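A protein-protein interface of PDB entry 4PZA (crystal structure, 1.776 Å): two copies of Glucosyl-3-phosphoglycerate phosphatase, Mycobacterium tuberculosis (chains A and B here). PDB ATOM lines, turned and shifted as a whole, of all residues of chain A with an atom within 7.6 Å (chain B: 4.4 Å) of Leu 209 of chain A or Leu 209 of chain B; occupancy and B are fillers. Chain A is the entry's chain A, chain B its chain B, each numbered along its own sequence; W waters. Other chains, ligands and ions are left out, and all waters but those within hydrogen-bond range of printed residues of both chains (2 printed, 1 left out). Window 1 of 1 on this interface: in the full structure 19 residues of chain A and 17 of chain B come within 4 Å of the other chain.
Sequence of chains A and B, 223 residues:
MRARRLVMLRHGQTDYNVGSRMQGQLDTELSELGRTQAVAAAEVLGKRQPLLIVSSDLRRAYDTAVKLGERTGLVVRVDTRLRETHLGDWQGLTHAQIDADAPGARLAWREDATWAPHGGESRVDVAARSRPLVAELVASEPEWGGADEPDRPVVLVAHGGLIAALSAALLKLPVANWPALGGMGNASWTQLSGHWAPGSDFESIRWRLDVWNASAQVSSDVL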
ATOM      1  N   ARG A 110      15.179   3.112 -29.622  1.00  0.00           N
ATOM      2  CA  ARG A 110      14.280   4.039 -28.942  1.00  0.00           C
ATOM      3  C   ARG A 110      12.895   4.133 -29.600  1.00  0.00           C
ATOM      4  O   ARG A 110      11.903   4.462 -28.938  1.00  0.00           O
ATOM      5  CB  ARG A 110      14.928   5.426 -28.909  1.00  0.00           C
ATOM      6  CG  ARG A 110      14.585   6.270 -27.692  1.00  0.00           C
ATOM      7  CD  ARG A 110      13.373   7.176 -27.923  1.00  0.00           C
ATOM      8  NE  ARG A 110      12.117   6.630 -27.395  1.00  0.00           N
ATOM      9  CZ  ARG A 110      11.824   6.524 -26.098  1.00  0.00           C
ATOM     10  NH1 ARG A 110      12.705   6.904 -25.174  1.00  0.00           N
ATOM     11  NH2 ARG A 110      10.653   6.021 -25.719  1.00  0.00           N
ATOM     12  N   SER A 167       4.486  -1.332 -18.124  1.00  0.00           N
ATOM     13  CA  SER A 167       3.374  -0.391 -18.041  1.00  0.00           C
ATOM     14  C   SER A 167       2.620  -0.360 -19.354  1.00  0.00           C
ATOM     15  O   SER A 167       1.402  -0.425 -19.368  1.00  0.00           O
ATOM     16  CB  SER A 167       3.847   1.020 -17.683  1.00  0.00           C
ATOM     17  OG  SER A 167       4.451   1.022 -16.401  1.00  0.00           O
ATOM     18  N   LEU A 171      -1.325  -1.344 -19.869  1.00  0.00           N
ATOM     19  CA  LEU A 171      -2.238  -0.323 -20.364  1.00  0.00           C
ATOM     20  C   LEU A 171      -2.834  -0.764 -21.682  1.00  0.00           C
ATOM     21  O   LEU A 171      -3.745  -0.120 -22.197  1.00  0.00           O
ATOM     22  CB  LEU A 171      -1.497   0.990 -20.599  1.00  0.00           C
ATOM     23  CG  LEU A 171      -0.973   1.701 -19.363  1.00  0.00           C
ATOM     24  CD1 LEU A 171      -0.078   2.828 -19.803  1.00  0.00           C
ATOM     25  CD2 LEU A 171      -2.137   2.236 -18.529  1.00  0.00           C
ATOM     26  N   LEU A 173      -1.496  -0.631 -24.678  1.00  0.00           N
ATOM     27  CA  LEU A 173      -1.116   0.175 -25.841  1.00  0.00           C
ATOM     28  C   LEU A 173      -0.691  -0.751 -26.974  1.00  0.00           C
ATOM     29  O   LEU A 173      -0.100  -1.804 -26.733  1.00  0.00           O
ATOM     30  CB  LEU A 173       0.043   1.098 -25.501  1.00  0.00           C
ATOM     31  CG  LEU A 173      -0.193   2.049 -24.340  1.00  0.00           C
ATOM     32  CD1 LEU A 173       1.077   2.870 -24.044  1.00  0.00           C
ATOM     33  CD2 LEU A 173      -1.386   2.955 -24.665  1.00  0.00           C
ATOM     34  N   PRO A 179       6.818   3.309 -27.524  1.00  0.00           N
ATOM     35  CA  PRO A 179       7.861   4.326 -27.309  1.00  0.00           C
ATOM     36  C   PRO A 179       7.364   5.698 -26.830  1.00  0.00           C
ATOM     37  O   PRO A 179       8.181   6.576 -26.578  1.00  0.00           O
ATOM     38  CB  PRO A 179       8.515   4.457 -28.693  1.00  0.00           C
ATOM     39  CG  PRO A 179       8.306   3.102 -29.330  1.00  0.00           C
ATOM     40  CD  PRO A 179       6.921   2.698 -28.869  1.00  0.00           C
ATOM     41  N   ALA A 180       6.056   5.881 -26.694  1.00  0.00           N
ATOM     42  CA  ALA A 180       5.534   7.132 -26.152  1.00  0.00           C
ATOM     43  C   ALA A 180       5.917   7.322 -24.680  1.00  0.00           C
ATOM     44  O   ALA A 180       5.892   8.446 -24.176  1.00  0.00           O
ATOM     45  CB  ALA A 180       4.027   7.216 -26.336  1.00  0.00           C
ATOM     46  N   LEU A 181       6.264   6.239 -23.987  1.00  0.00           N
ATOM     47  CA  LEU A 181       6.669   6.361 -22.578  1.00  0.00           C
ATOM     48  C   LEU A 181       8.149   6.684 -22.464  1.00  0.00           C
ATOM     49  O   LEU A 181       9.009   5.870 -22.830  1.00  0.00           O
ATOM     50  CB  LEU A 181       6.341   5.101 -21.773  1.00  0.00           C
ATOM     51  CG  LEU A 181       4.860   4.752 -21.620  1.00  0.00           C
ATOM     52  CD1 LEU A 181       4.640   3.504 -20.758  1.00  0.00           C
ATOM     53  CD2 LEU A 181       4.088   5.927 -21.050  1.00  0.00           C
ATOM     54  N   GLY A 182       8.438   7.882 -21.965  1.00  0.00           N
ATOM     55  CA  GLY A 182       9.801   8.337 -21.758  1.00  0.00           C
ATOM     56  C   GLY A 182      10.560   7.540 -20.719  1.00  0.00           C
ATOM     57  O   GLY A 182      10.107   6.490 -20.263  1.00  0.00           O
ATOM     58  N   GLY A 183      11.742   8.023 -20.362  1.00  0.00           N
ATOM     59  CA  GLY A 183      12.585   7.289 -19.442  1.00  0.00           C
ATOM     60  C   GLY A 183      12.397   7.779 -18.027  1.00  0.00           C
ATOM     61  O   GLY A 183      12.294   8.983 -17.790  1.00  0.00           O
ATOM     62  N   MET A 184      12.358   6.842 -17.088  1.00  0.00           N
ATOM     63  CA  MET A 184      12.279   7.151 -15.662  1.00  0.00           C
ATOM     64  C   MET A 184      13.589   7.728 -15.132  1.00  0.00           C
ATOM     65  O   MET A 184      14.666   7.219 -15.452  1.00  0.00           O
ATOM     66  CB  MET A 184      11.990   5.868 -14.885  1.00  0.00           C
ATOM     67  CG  MET A 184      10.714   5.141 -15.278  1.00  0.00           C
ATOM     68  SD  MET A 184       9.225   5.854 -14.551  1.00  0.00           S
ATOM     69  CE  MET A 184       9.463   5.457 -12.786  1.00  0.00           C
ATOM     70  N   THR A 190       6.204   5.545 -10.621  1.00  0.00           N
ATOM     71  CA  THR A 190       5.083   5.498 -11.557  1.00  0.00           C
ATOM     72  C   THR A 190       3.970   4.736 -10.862  1.00  0.00           C
ATOM     73  O   THR A 190       4.238   3.850 -10.032  1.00  0.00           O
ATOM     74  CB  THR A 190       5.517   4.791 -12.851  1.00  0.00           C
ATOM     75  OG1 THR A 190       6.243   5.721 -13.653  1.00  0.00           O
ATOM     76  CG2 THR A 190       4.319   4.240 -13.669  1.00  0.00           C
ATOM     77  N   GLN A 191       2.723   5.090 -11.156  1.00  0.00           N
ATOM     78  CA  GLN A 191       1.587   4.376 -10.575  1.00  0.00           C
ATOM     79  C   GLN A 191       0.528   4.111 -11.622  1.00  0.00           C
ATOM     80  O   GLN A 191       0.158   5.029 -12.365  1.00  0.00           O
ATOM     81  CB  GLN A 191       0.970   5.189  -9.448  1.00  0.00           C
ATOM     82  CG  GLN A 191      -0.252   4.519  -8.871  1.00  0.00           C
ATOM     83  CD  GLN A 191      -0.790   5.241  -7.664  1.00  0.00           C
ATOM     84  OE1 GLN A 191      -0.091   5.404  -6.654  1.00  0.00           O
ATOM     85  NE2 GLN A 191      -2.043   5.665  -7.744  1.00  0.00           N
ATOM     86  N   LEU A 192       0.082   2.853 -11.713  1.00  0.00           N
ATOM     87  CA  LEU A 192      -1.057   2.488 -12.549  1.00  0.00           C
ATOM     88  C   LEU A 192      -2.170   2.088 -11.593  1.00  0.00           C
ATOM     89  O   LEU A 192      -1.900   1.636 -10.476  1.00  0.00           O
ATOM     90  CB  LEU A 192      -0.722   1.274 -13.438  1.00  0.00           C
ATOM     91  CG  LEU A 192      -0.071   1.534 -14.809  1.00  0.00           C
ATOM     92  CD1 LEU A 192       1.245   2.226 -14.672  1.00  0.00           C
ATOM     93  CD2 LEU A 192       0.117   0.233 -15.581  1.00  0.00           C
ATOM     94  N   SER A 193      -3.415   2.235 -12.016  1.00  0.00           N
ATOM     95  CA  SER A 193      -4.518   1.690 -11.229  1.00  0.00           C
ATOM     96  C   SER A 193      -5.353   0.763 -12.098  1.00  0.00           C
ATOM     97  O   SER A 193      -5.659   1.078 -13.257  1.00  0.00           O
ATOM     98  CB  SER A 193      -5.351   2.800 -10.579  1.00  0.00           C
ATOM     99  OG  SER A 193      -5.867   3.696 -11.549  1.00  0.00           O
ATOM    100  N   HIS A 195      -8.789  -1.133 -12.724  1.00  0.00           N
ATOM    101  CA  HIS A 195     -10.212  -1.006 -12.425  1.00  0.00           C
ATOM    102  C   HIS A 195     -10.990  -2.155 -13.054  1.00  0.00           C
ATOM    103  O   HIS A 195     -10.698  -2.571 -14.173  1.00  0.00           O
ATOM    104  CB  HIS A 195     -10.755   0.320 -12.987  1.00  0.00           C
ATOM    105  CG  HIS A 195     -10.051   1.533 -12.468  1.00  0.00           C
ATOM    106  ND1 HIS A 195     -10.612   2.384 -11.535  1.00  0.00           N
ATOM    107  CD2 HIS A 195      -8.819   2.031 -12.731  1.00  0.00           C
ATOM    108  CE1 HIS A 195      -9.762   3.352 -11.257  1.00  0.00           C
ATOM    109  NE2 HIS A 195      -8.662   3.159 -11.967  1.00  0.00           N
ATOM    110  N   ARG A 206      -9.059  -3.160 -16.291  1.00  0.00           N
ATOM    111  CA  ARG A 206      -8.609  -2.105 -17.196  1.00  0.00           C
ATOM    112  C   ARG A 206      -7.639  -1.199 -16.464  1.00  0.00           C
ATOM    113  O   ARG A 206      -8.020  -0.544 -15.487  1.00  0.00           O
ATOM    114  CB  ARG A 206      -9.791  -1.265 -17.680  1.00  0.00           C
ATOM    115  CG  ARG A 206     -10.651  -1.932 -18.732  1.00  0.00           C
ATOM    116  CD  ARG A 206     -11.959  -1.180 -18.882  1.00  0.00           C
ATOM    117  NE  ARG A 206     -12.439  -1.168 -20.263  1.00  0.00           N
ATOM    118  CZ  ARG A 206     -13.642  -0.729 -20.624  1.00  0.00           C
ATOM    119  NH1 ARG A 206     -14.486  -0.277 -19.702  1.00  0.00           N
ATOM    120  NH2 ARG A 206     -14.006  -0.744 -21.902  1.00  0.00           N
ATOM    121  N   TRP A 207      -6.394  -1.140 -16.929  1.00  0.00           N
ATOM    122  CA  TRP A 207      -5.386  -0.330 -16.240  1.00  0.00           C
ATOM    123  C   TRP A 207      -5.319   1.082 -16.806  1.00  0.00           C
ATOM    124  O   TRP A 207      -5.467   1.282 -18.022  1.00  0.00           O
ATOM    125  CB  TRP A 207      -4.014  -1.011 -16.355  1.00  0.00           C
ATOM    126  CG  TRP A 207      -3.971  -2.357 -15.672  1.00  0.00           C
ATOM    127  CD1 TRP A 207      -4.299  -3.568 -16.219  1.00  0.00           C
ATOM    128  CD2 TRP A 207      -3.594  -2.620 -14.315  1.00  0.00           C
ATOM    129  NE1 TRP A 207      -4.140  -4.563 -15.288  1.00  0.00           N
ATOM    130  CE2 TRP A 207      -3.712  -4.007 -14.109  1.00  0.00           C
ATOM    131  CE3 TRP A 207      -3.173  -1.812 -13.251  1.00  0.00           C
ATOM    132  CZ2 TRP A 207      -3.416  -4.610 -12.879  1.00  0.00           C
ATOM    133  CZ3 TRP A 207      -2.878  -2.411 -12.030  1.00  0.00           C
ATOM    134  CH2 TRP A 207      -3.005  -3.792 -11.857  1.00  0.00           C
ATOM    135  N   ARG A 208      -5.132   2.070 -15.928  1.00  0.00           N
ATOM    136  CA  ARG A 208      -4.898   3.440 -16.378  1.00  0.00           C
ATOM    137  C   ARG A 208      -3.645   4.011 -15.736  1.00  0.00           C
ATOM    138  O   ARG A 208      -3.207   3.550 -14.676  1.00  0.00           O
ATOM    139  CB  ARG A 208      -6.109   4.353 -16.112  1.00  0.00           C
ATOM    140  CG  ARG A 208      -6.308   4.709 -14.659  1.00  0.00           C
ATOM    141  CD  ARG A 208      -7.580   5.554 -14.459  1.00  0.00           C
ATOM    142  NE  ARG A 208      -8.786   4.767 -14.722  1.00  0.00           N
ATOM    143  CZ  ARG A 208     -10.006   5.093 -14.300  1.00  0.00           C
ATOM    144  NH1 ARG A 208     -10.195   6.197 -13.592  1.00  0.00           N
ATOM    145  NH2 ARG A 208     -11.039   4.310 -14.589  1.00  0.00           N
ATOM    146  N   LEU A 209      -3.049   5.004 -16.396  1.00  0.00           N
ATOM    147  CA  LEU A 209      -1.811   5.602 -15.906  1.00  0.00           C
ATOM    148  C   LEU A 209      -2.115   6.770 -14.960  1.00  0.00           C
ATOM    149  O   LEU A 209      -2.619   7.798 -15.401  1.00  0.00           O
ATOM    150  CB  LEU A 209      -0.954   6.058 -17.112  1.00  0.00           C
ATOM    151  CG  LEU A 209       0.363   6.770 -16.797  1.00  0.00           C
ATOM    152  CD1 LEU A 209       1.282   5.842 -15.981  1.00  0.00           C
ATOM    153  CD2 LEU A 209       1.072   7.214 -18.064  1.00  0.00           C
ATOM    154  N   ASP A 210      -1.814   6.610 -13.663  1.00  0.00           N
ATOM    155  CA  ASP A 210      -2.092   7.657 -12.673  1.00  0.00           C
ATOM    156  C   ASP A 210      -0.954   8.667 -12.592  1.00  0.00           C
ATOM    157  O   ASP A 210      -1.191   9.871 -12.497  1.00  0.00           O
ATOM    158  CB  ASP A 210      -2.265   7.073 -11.261  1.00  0.00           C
ATOM    159  CG  ASP A 210      -3.483   6.173 -11.118  1.00  0.00           C
ATOM    160  OD1 ASP A 210      -4.453   6.278 -11.911  1.00  0.00           O
ATOM    161  OD2 ASP A 210      -3.477   5.362 -10.167  1.00  0.00           O
ATOM    162  N   VAL A 211       0.274   8.152 -12.586  1.00  0.00           N
ATOM    163  CA  VAL A 211       1.484   8.947 -12.414  1.00  0.00           C
ATOM    164  C   VAL A 211       2.590   8.310 -13.239  1.00  0.00           C
ATOM    165  O   VAL A 211       2.773   7.084 -13.197  1.00  0.00           O
ATOM    166  CB  VAL A 211       1.936   8.933 -10.921  1.00  0.00           C
ATOM    167  CG1 VAL A 211       3.271   9.655 -10.733  1.00  0.00           C
ATOM    168  CG2 VAL A 211       0.875   9.584 -10.028  1.00  0.00           C
ATOM    169  N   TRP A 212       3.326   9.117 -13.991  1.00  0.00           N
ATOM    170  CA  TRP A 212       4.513   8.612 -14.691  1.00  0.00           C
ATOM    171  C   TRP A 212       5.732   9.464 -14.352  1.00  0.00           C
ATOM    172  O   TRP A 212       5.731  10.686 -14.560  1.00  0.00           O
ATOM    173  CB  TRP A 212       4.301   8.549 -16.225  1.00  0.00           C
ATOM    174  CG  TRP A 212       5.560   8.110 -16.940  1.00  0.00           C
ATOM    175  CD1 TRP A 212       6.508   8.913 -17.501  1.00  0.00           C
ATOM    176  CD2 TRP A 212       6.018   6.764 -17.123  1.00  0.00           C
ATOM    177  NE1 TRP A 212       7.529   8.154 -18.025  1.00  0.00           N
ATOM    178  CE2 TRP A 212       7.248   6.831 -17.810  1.00  0.00           C
ATOM    179  CE3 TRP A 212       5.506   5.509 -16.769  1.00  0.00           C
ATOM    180  CZ2 TRP A 212       7.973   5.690 -18.154  1.00  0.00           C
ATOM    181  CZ3 TRP A 212       6.229   4.378 -17.101  1.00  0.00           C
ATOM    182  CH2 TRP A 212       7.449   4.476 -17.793  1.00  0.00           C
ATOM    183  N   ASN A 213       6.763   8.827 -13.791  1.00  0.00           N
ATOM    184  CA  ASN A 213       8.049   9.493 -13.566  1.00  0.00           C
ATOM    185  C   ASN A 213       7.976  10.723 -12.647  1.00  0.00           C
ATOM    186  O   ASN A 213       8.505  11.792 -12.978  1.00  0.00           O
ATOM    187  CB  ASN A 213       8.732   9.827 -14.904  1.00  0.00           C
ATOM    188  CG  ASN A 213      10.162  10.313 -14.730  1.00  0.00           C
ATOM    189  OD1 ASN A 213      10.854   9.918 -13.788  1.00  0.00           O
ATOM    190  ND2 ASN A 213      10.608  11.184 -15.633  1.00  0.00           N
ATOM    191  N   LEU B 171       0.952  12.621 -28.572  1.00  0.00           N
ATOM    192  CA  LEU B 171       1.671  11.355 -28.519  1.00  0.00           C
ATOM    193  C   LEU B 171       1.247  10.436 -29.653  1.00  0.00           C
ATOM    194  O   LEU B 171       1.838   9.360 -29.849  1.00  0.00           O
ATOM    195  CB  LEU B 171       1.397  10.653 -27.192  1.00  0.00           C
ATOM    196  CG  LEU B 171       1.950  11.328 -25.942  1.00  0.00           C
ATOM    197  CD1 LEU B 171       1.388  10.653 -24.719  1.00  0.00           C
ATOM    198  CD2 LEU B 171       3.486  11.279 -25.909  1.00  0.00           C
ATOM    199  N   ALA B 180      -6.288   5.379 -21.446  1.00  0.00           N
ATOM    200  CA  ALA B 180      -5.128   4.926 -20.680  1.00  0.00           C
ATOM    201  C   ALA B 180      -4.543   6.046 -19.806  1.00  0.00           C
ATOM    202  O   ALA B 180      -3.910   5.773 -18.782  1.00  0.00           O
ATOM    203  CB  ALA B 180      -4.074   4.360 -21.608  1.00  0.00           C
ATOM    204  N   LEU B 181      -4.734   7.305 -20.199  1.00  0.00           N
ATOM    205  CA  LEU B 181      -4.265   8.412 -19.354  1.00  0.00           C
ATOM    206  C   LEU B 181      -5.270   8.708 -18.255  1.00  0.00           C
ATOM    207  O   LEU B 181      -6.443   8.979 -18.524  1.00  0.00           O
ATOM    208  CB  LEU B 181      -3.981   9.680 -20.162  1.00  0.00           C
ATOM    209  CG  LEU B 181      -2.845   9.606 -21.182  1.00  0.00           C
ATOM    210  CD1 LEU B 181      -2.607  10.940 -21.879  1.00  0.00           C
ATOM    211  CD2 LEU B 181      -1.573   9.140 -20.505  1.00  0.00           C
ATOM    212  N   GLY B 182      -4.803   8.658 -17.013  1.00  0.00           N
ATOM    213  CA  GLY B 182      -5.650   8.883 -15.858  1.00  0.00           C
ATOM    214  C   GLY B 182      -5.850  10.364 -15.622  1.00  0.00           C
ATOM    215  O   GLY B 182      -5.750  11.175 -16.551  1.00  0.00           O
ATOM    216  N   THR B 190       2.661  17.916 -15.999  1.00  0.00           N
ATOM    217  CA  THR B 190       2.961  16.907 -17.007  1.00  0.00           C
ATOM    218  C   THR B 190       3.951  17.550 -17.967  1.00  0.00           C
ATOM    219  O   THR B 190       3.908  18.777 -18.186  1.00  0.00           O
ATOM    220  CB  THR B 190       1.672  16.499 -17.721  1.00  0.00           C
ATOM    221  OG1 THR B 190       0.953  15.589 -16.879  1.00  0.00           O
ATOM    222  CG2 THR B 190       1.940  15.832 -19.093  1.00  0.00           C
ATOM    223  N   GLN B 191       4.883  16.754 -18.483  1.00  0.00           N
ATOM    224  CA  GLN B 191       5.811  17.233 -19.500  1.00  0.00           C
ATOM    225  C   GLN B 191       5.921  16.254 -20.658  1.00  0.00           C
ATOM    226  O   GLN B 191       6.078  15.049 -20.438  1.00  0.00           O
ATOM    227  CB  GLN B 191       7.194  17.443 -18.902  1.00  0.00           C
ATOM    228  CG  GLN B 191       8.233  17.935 -19.900  1.00  0.00           C
ATOM    229  CD  GLN B 191       9.563  18.233 -19.223  1.00  0.00           C
ATOM    230  OE1 GLN B 191       9.672  19.168 -18.415  1.00  0.00           O
ATOM    231  NE2 GLN B 191      10.580  17.428 -19.531  1.00  0.00           N
ATOM    232  N   LEU B 192       5.813  16.786 -21.876  1.00  0.00           N
ATOM    233  CA  LEU B 192       6.109  16.053 -23.103  1.00  0.00           C
ATOM    234  C   LEU B 192       7.345  16.688 -23.724  1.00  0.00           C
ATOM    235  O   LEU B 192       7.587  17.892 -23.558  1.00  0.00           O
ATOM    236  CB  LEU B 192       4.945  16.179 -24.102  1.00  0.00           C
ATOM    237  CG  LEU B 192       3.787  15.183 -23.921  1.00  0.00           C
ATOM    238  CD1 LEU B 192       3.044  15.409 -22.626  1.00  0.00           C
ATOM    239  CD2 LEU B 192       2.794  15.248 -25.091  1.00  0.00           C
ATOM    240  N   ARG B 208       7.172  12.555 -26.823  1.00  0.00           N
ATOM    241  CA  ARG B 208       7.354  11.501 -25.838  1.00  0.00           C
ATOM    242  C   ARG B 208       6.829  12.000 -24.496  1.00  0.00           C
ATOM    243  O   ARG B 208       6.938  13.187 -24.194  1.00  0.00           O
ATOM    244  CB  ARG B 208       8.849  11.172 -25.741  1.00  0.00           C
ATOM    245  CG  ARG B 208       9.211  10.029 -24.834  1.00  0.00           C
ATOM    246  CD  ARG B 208      10.733   9.869 -24.816  1.00  0.00           C
ATOM    247  NE  ARG B 208      11.298  10.012 -26.157  1.00  0.00           N
ATOM    248  CZ  ARG B 208      12.591  10.212 -26.409  1.00  0.00           C
ATOM    249  NH1 ARG B 208      13.461  10.298 -25.407  1.00  0.00           N
ATOM    250  NH2 ARG B 208      13.014  10.328 -27.662  1.00  0.00           N
ATOM    251  N   LEU B 209       6.257  11.106 -23.687  1.00  0.00           N
ATOM    252  CA  LEU B 209       5.770  11.509 -22.364  1.00  0.00           C
ATOM    253  C   LEU B 209       6.896  11.424 -21.340  1.00  0.00           C
ATOM    254  O   LEU B 209       7.356  10.322 -21.021  1.00  0.00           O
ATOM    255  CB  LEU B 209       4.594  10.614 -21.940  1.00  0.00           C
ATOM    256  CG  LEU B 209       3.960  10.806 -20.554  1.00  0.00           C
ATOM    257  CD1 LEU B 209       3.348  12.190 -20.394  1.00  0.00           C
ATOM    258  CD2 LEU B 209       2.901   9.736 -20.300  1.00  0.00           C
ATOM    259  N   ASP B 210       7.344  12.576 -20.825  1.00  0.00           N
ATOM    260  CA  ASP B 210       8.442  12.599 -19.857  1.00  0.00           C
ATOM    261  C   ASP B 210       7.961  12.421 -18.416  1.00  0.00           C
ATOM    262  O   ASP B 210       8.574  11.685 -17.632  1.00  0.00           O
ATOM    263  CB  ASP B 210       9.214  13.927 -19.913  1.00  0.00           C
ATOM    264  CG  ASP B 210       9.892  14.182 -21.258  1.00  0.00           C
ATOM    265  OD1 ASP B 210      10.195  13.232 -22.011  1.00  0.00           O
ATOM    266  OD2 ASP B 210      10.126  15.373 -21.556  1.00  0.00           O
ATOM    267  N   VAL B 211       6.878  13.127 -18.075  1.00  0.00           N
ATOM    268  CA  VAL B 211       6.307  13.137 -16.735  1.00  0.00           C
ATOM    269  C   VAL B 211       4.789  13.239 -16.876  1.00  0.00           C
ATOM    270  O   VAL B 211       4.299  14.049 -17.660  1.00  0.00           O
ATOM    271  CB  VAL B 211       6.783  14.383 -15.939  1.00  0.00           C
ATOM    272  CG1 VAL B 211       6.104  14.460 -14.592  1.00  0.00           C
ATOM    273  CG2 VAL B 211       8.293  14.375 -15.741  1.00  0.00           C
ATOM    274  N   TRP B 212       4.044  12.418 -16.139  1.00  0.00           N
ATOM    275  CA  TRP B 212       2.589  12.565 -16.089  1.00  0.00           C
ATOM    276  C   TRP B 212       2.144  12.691 -14.638  1.00  0.00           C
ATOM    277  O   TRP B 212       2.396  11.804 -13.827  1.00  0.00           O
ATOM    278  CB  TRP B 212       1.861  11.376 -16.771  1.00  0.00           C
ATOM    279  CG  TRP B 212       0.362  11.475 -16.596  1.00  0.00           C
ATOM    280  CD1 TRP B 212      -0.401  10.886 -15.629  1.00  0.00           C
ATOM    281  CD2 TRP B 212      -0.539  12.245 -17.399  1.00  0.00           C
ATOM    282  NE1 TRP B 212      -1.730  11.245 -15.786  1.00  0.00           N
ATOM    283  CE2 TRP B 212      -1.832  12.075 -16.866  1.00  0.00           C
ATOM    284  CE3 TRP B 212      -0.375  13.067 -18.523  1.00  0.00           C
ATOM    285  CZ2 TRP B 212      -2.957  12.695 -17.421  1.00  0.00           C
ATOM    286  CZ3 TRP B 212      -1.484  13.684 -19.060  1.00  0.00           C
ATOM    287  CH2 TRP B 212      -2.762  13.496 -18.509  1.00  0.00           C
HETATM  288  O   HOH W   1      11.739  11.200 -21.313  1.00  0.00           O
HETATM  289  O   HOH W   2      11.332  11.083 -18.754  1.00  0.00           O
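The backbone NH (N) of Gly 182 of chain A is in hydrogen-bond range of the backbone carbonyl oxygen (O) of Leu 209 of chain B.
O of Asp 210 of chain B lies within hydrogen-bond range of ND2 of Asn 213 of chain A (2.9 Å).
The backbone NH of Leu 209 of chain A lies within hydrogen-bond range of the backbone carbonyl oxygen of Ala 180 of chain B, 2.7 Å away.
The backbone carbonyl oxygen of Leu 209 of chain A is in hydrogen-bond range of the backbone NH of Gly 182 of chain B (2.8 Å).
NH1 of Arg 208 of chain B sits close to NH1 of Arg 110 of chain A (3.5 Å).
The backbone NH (N) of Leu 209 of chain B lies within hydrogen-bond range of the backbone carbonyl oxygen (O) of Ala 180 of chain A, at 2.7 Å.
The backbone carbonyl oxygen (O) of Trp 212 of chain B is in hydrogen-bond range of the backbone NH (N) of Trp 212 of chain A.
OG1 of Thr 190 of chain A is in hydrogen-bond range of N of Asn 213 of chain A.
NH2 of Arg 110 of chain A lies within hydrogen-bond range of O of Leu 181 of chain A, at 3.3 Å.
The backbone carbonyl oxygen of Val 211 of chain B is in hydrogen-bond range of the backbone NH of Gln 191 of chain B (2.9 Å).
The backbone carbonyl oxygen (O) of Pro 179 of chain A is in hydrogen-bond range of the guanidinium group (NH2) of Arg 110 of chain A (2.7 Å).
Among the printed residues, merely in contact across the chains: Leu 171 of chain A with Ala 180 of chain B (3.96 Å), Ala 180 of chain A with Arg 208 of chain B (3.7 Å), Leu 181 of chain A with Leu 209 of chain B (3.99 Å), Gly 182 of chain A with Arg 208 of chain B (3.5 Å), Arg 208 of chain A with Ala 180 of chain B (3.5 Å), Leu 209 of chain A with Leu 209 of chain B (3.8 Å), Leu 209 of chain A with Trp 212 of chain B (3.6 Å), Asp 210 of chain A with Trp 212 of chain B (3.4 Å), Val 211 of chain A with Trp 212 of chain B (3.3 Å), Trp 212 of chain A with Leu 209 of chain B (3.7 Å), Trp 212 of chain A with Asp 210 of chain B (3.5 Å), Trp 212 of chain A with Val 211 of chain B (3.3 Å) and Asn 213 of chain A with Val 211 of chain B (3.8 Å).
Of the printed residues of chain B, Leu 209 of chain A touches Ala 180, Gly 182, Leu 209 and Trp 212.
Printed residues of chain B within 4 Å of Arg 208 of chain A: Ala 180.
Of the printed residues of chain A, Arg 208 of chain B touches Arg 110 (3.2 Å), Ala 180 (3.7 Å) and Gly 182 (3.5 Å).
Printed residues of chain A within 4 Å of Trp 212 of chain B: Leu 209 (3.6 Å), Asp 210 (3.4 Å), Val 211 (3.3 Å) and Trp 212 (2.8 Å).
Printed residues of chain B within 4 Å of Asp 210 of chain A: Trp 212.
The nearest printed residue of chain B that does not touch Leu 209 of chain A is Leu 181 of chain B (4.0002 Å).
The nearest printed residue of chain A that does not touch Leu 209 of chain B is Gly 183 of chain A (5.0 Å).
The nearest printed residue of chain B that does not touch Gly 182 of chain A is Asp 210 of chain B (4.9 Å).
Of the 23 printed residues of chain A, 11 touch a printed residue of chain B.
Hydrophobic or aromatic side chains of chain A that line the printed part of chain B: Leu 171, Leu 209, Val 211 and Trp 212.
Hydrophobic or aromatic side chains of chain B that line the printed part of chain A: Leu 209, Val 211 and Trp 212.
Ala 180 of chain A touches Leu 209 of chain B, and with the chains exchanged Leu 209 of chain A touches Ala 180 of chain B.
Leu 181 of chain A touches Leu 209 of chain B, but with the chains exchanged Leu 209 of chain A does not touch Leu 181 of chain B (4.0002 Å).
Gly 182 of chain A touches Arg 208 of chain B, but with the chains exchanged Arg 208 of chain A does not touch Gly 182 of chain B (4.1 Å).
12 positions are printed for both chains.
Water W2 lies within hydrogen-bond range of the backbone carbonyl oxygen (O) of Gly 183 of chain A, the backbone carbonyl oxygen (O) of Asp 210 of chain B and the side-chain amide nitrogen (ND2) of Asn 213 of chain A.
Water W1 lies within hydrogen-bond range of the side-chain carboxylate (OD1) of Asp 210 of chain B (2.6 Å) and the backbone NH (N) of Gly 183 of chain A (3.3 Å).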
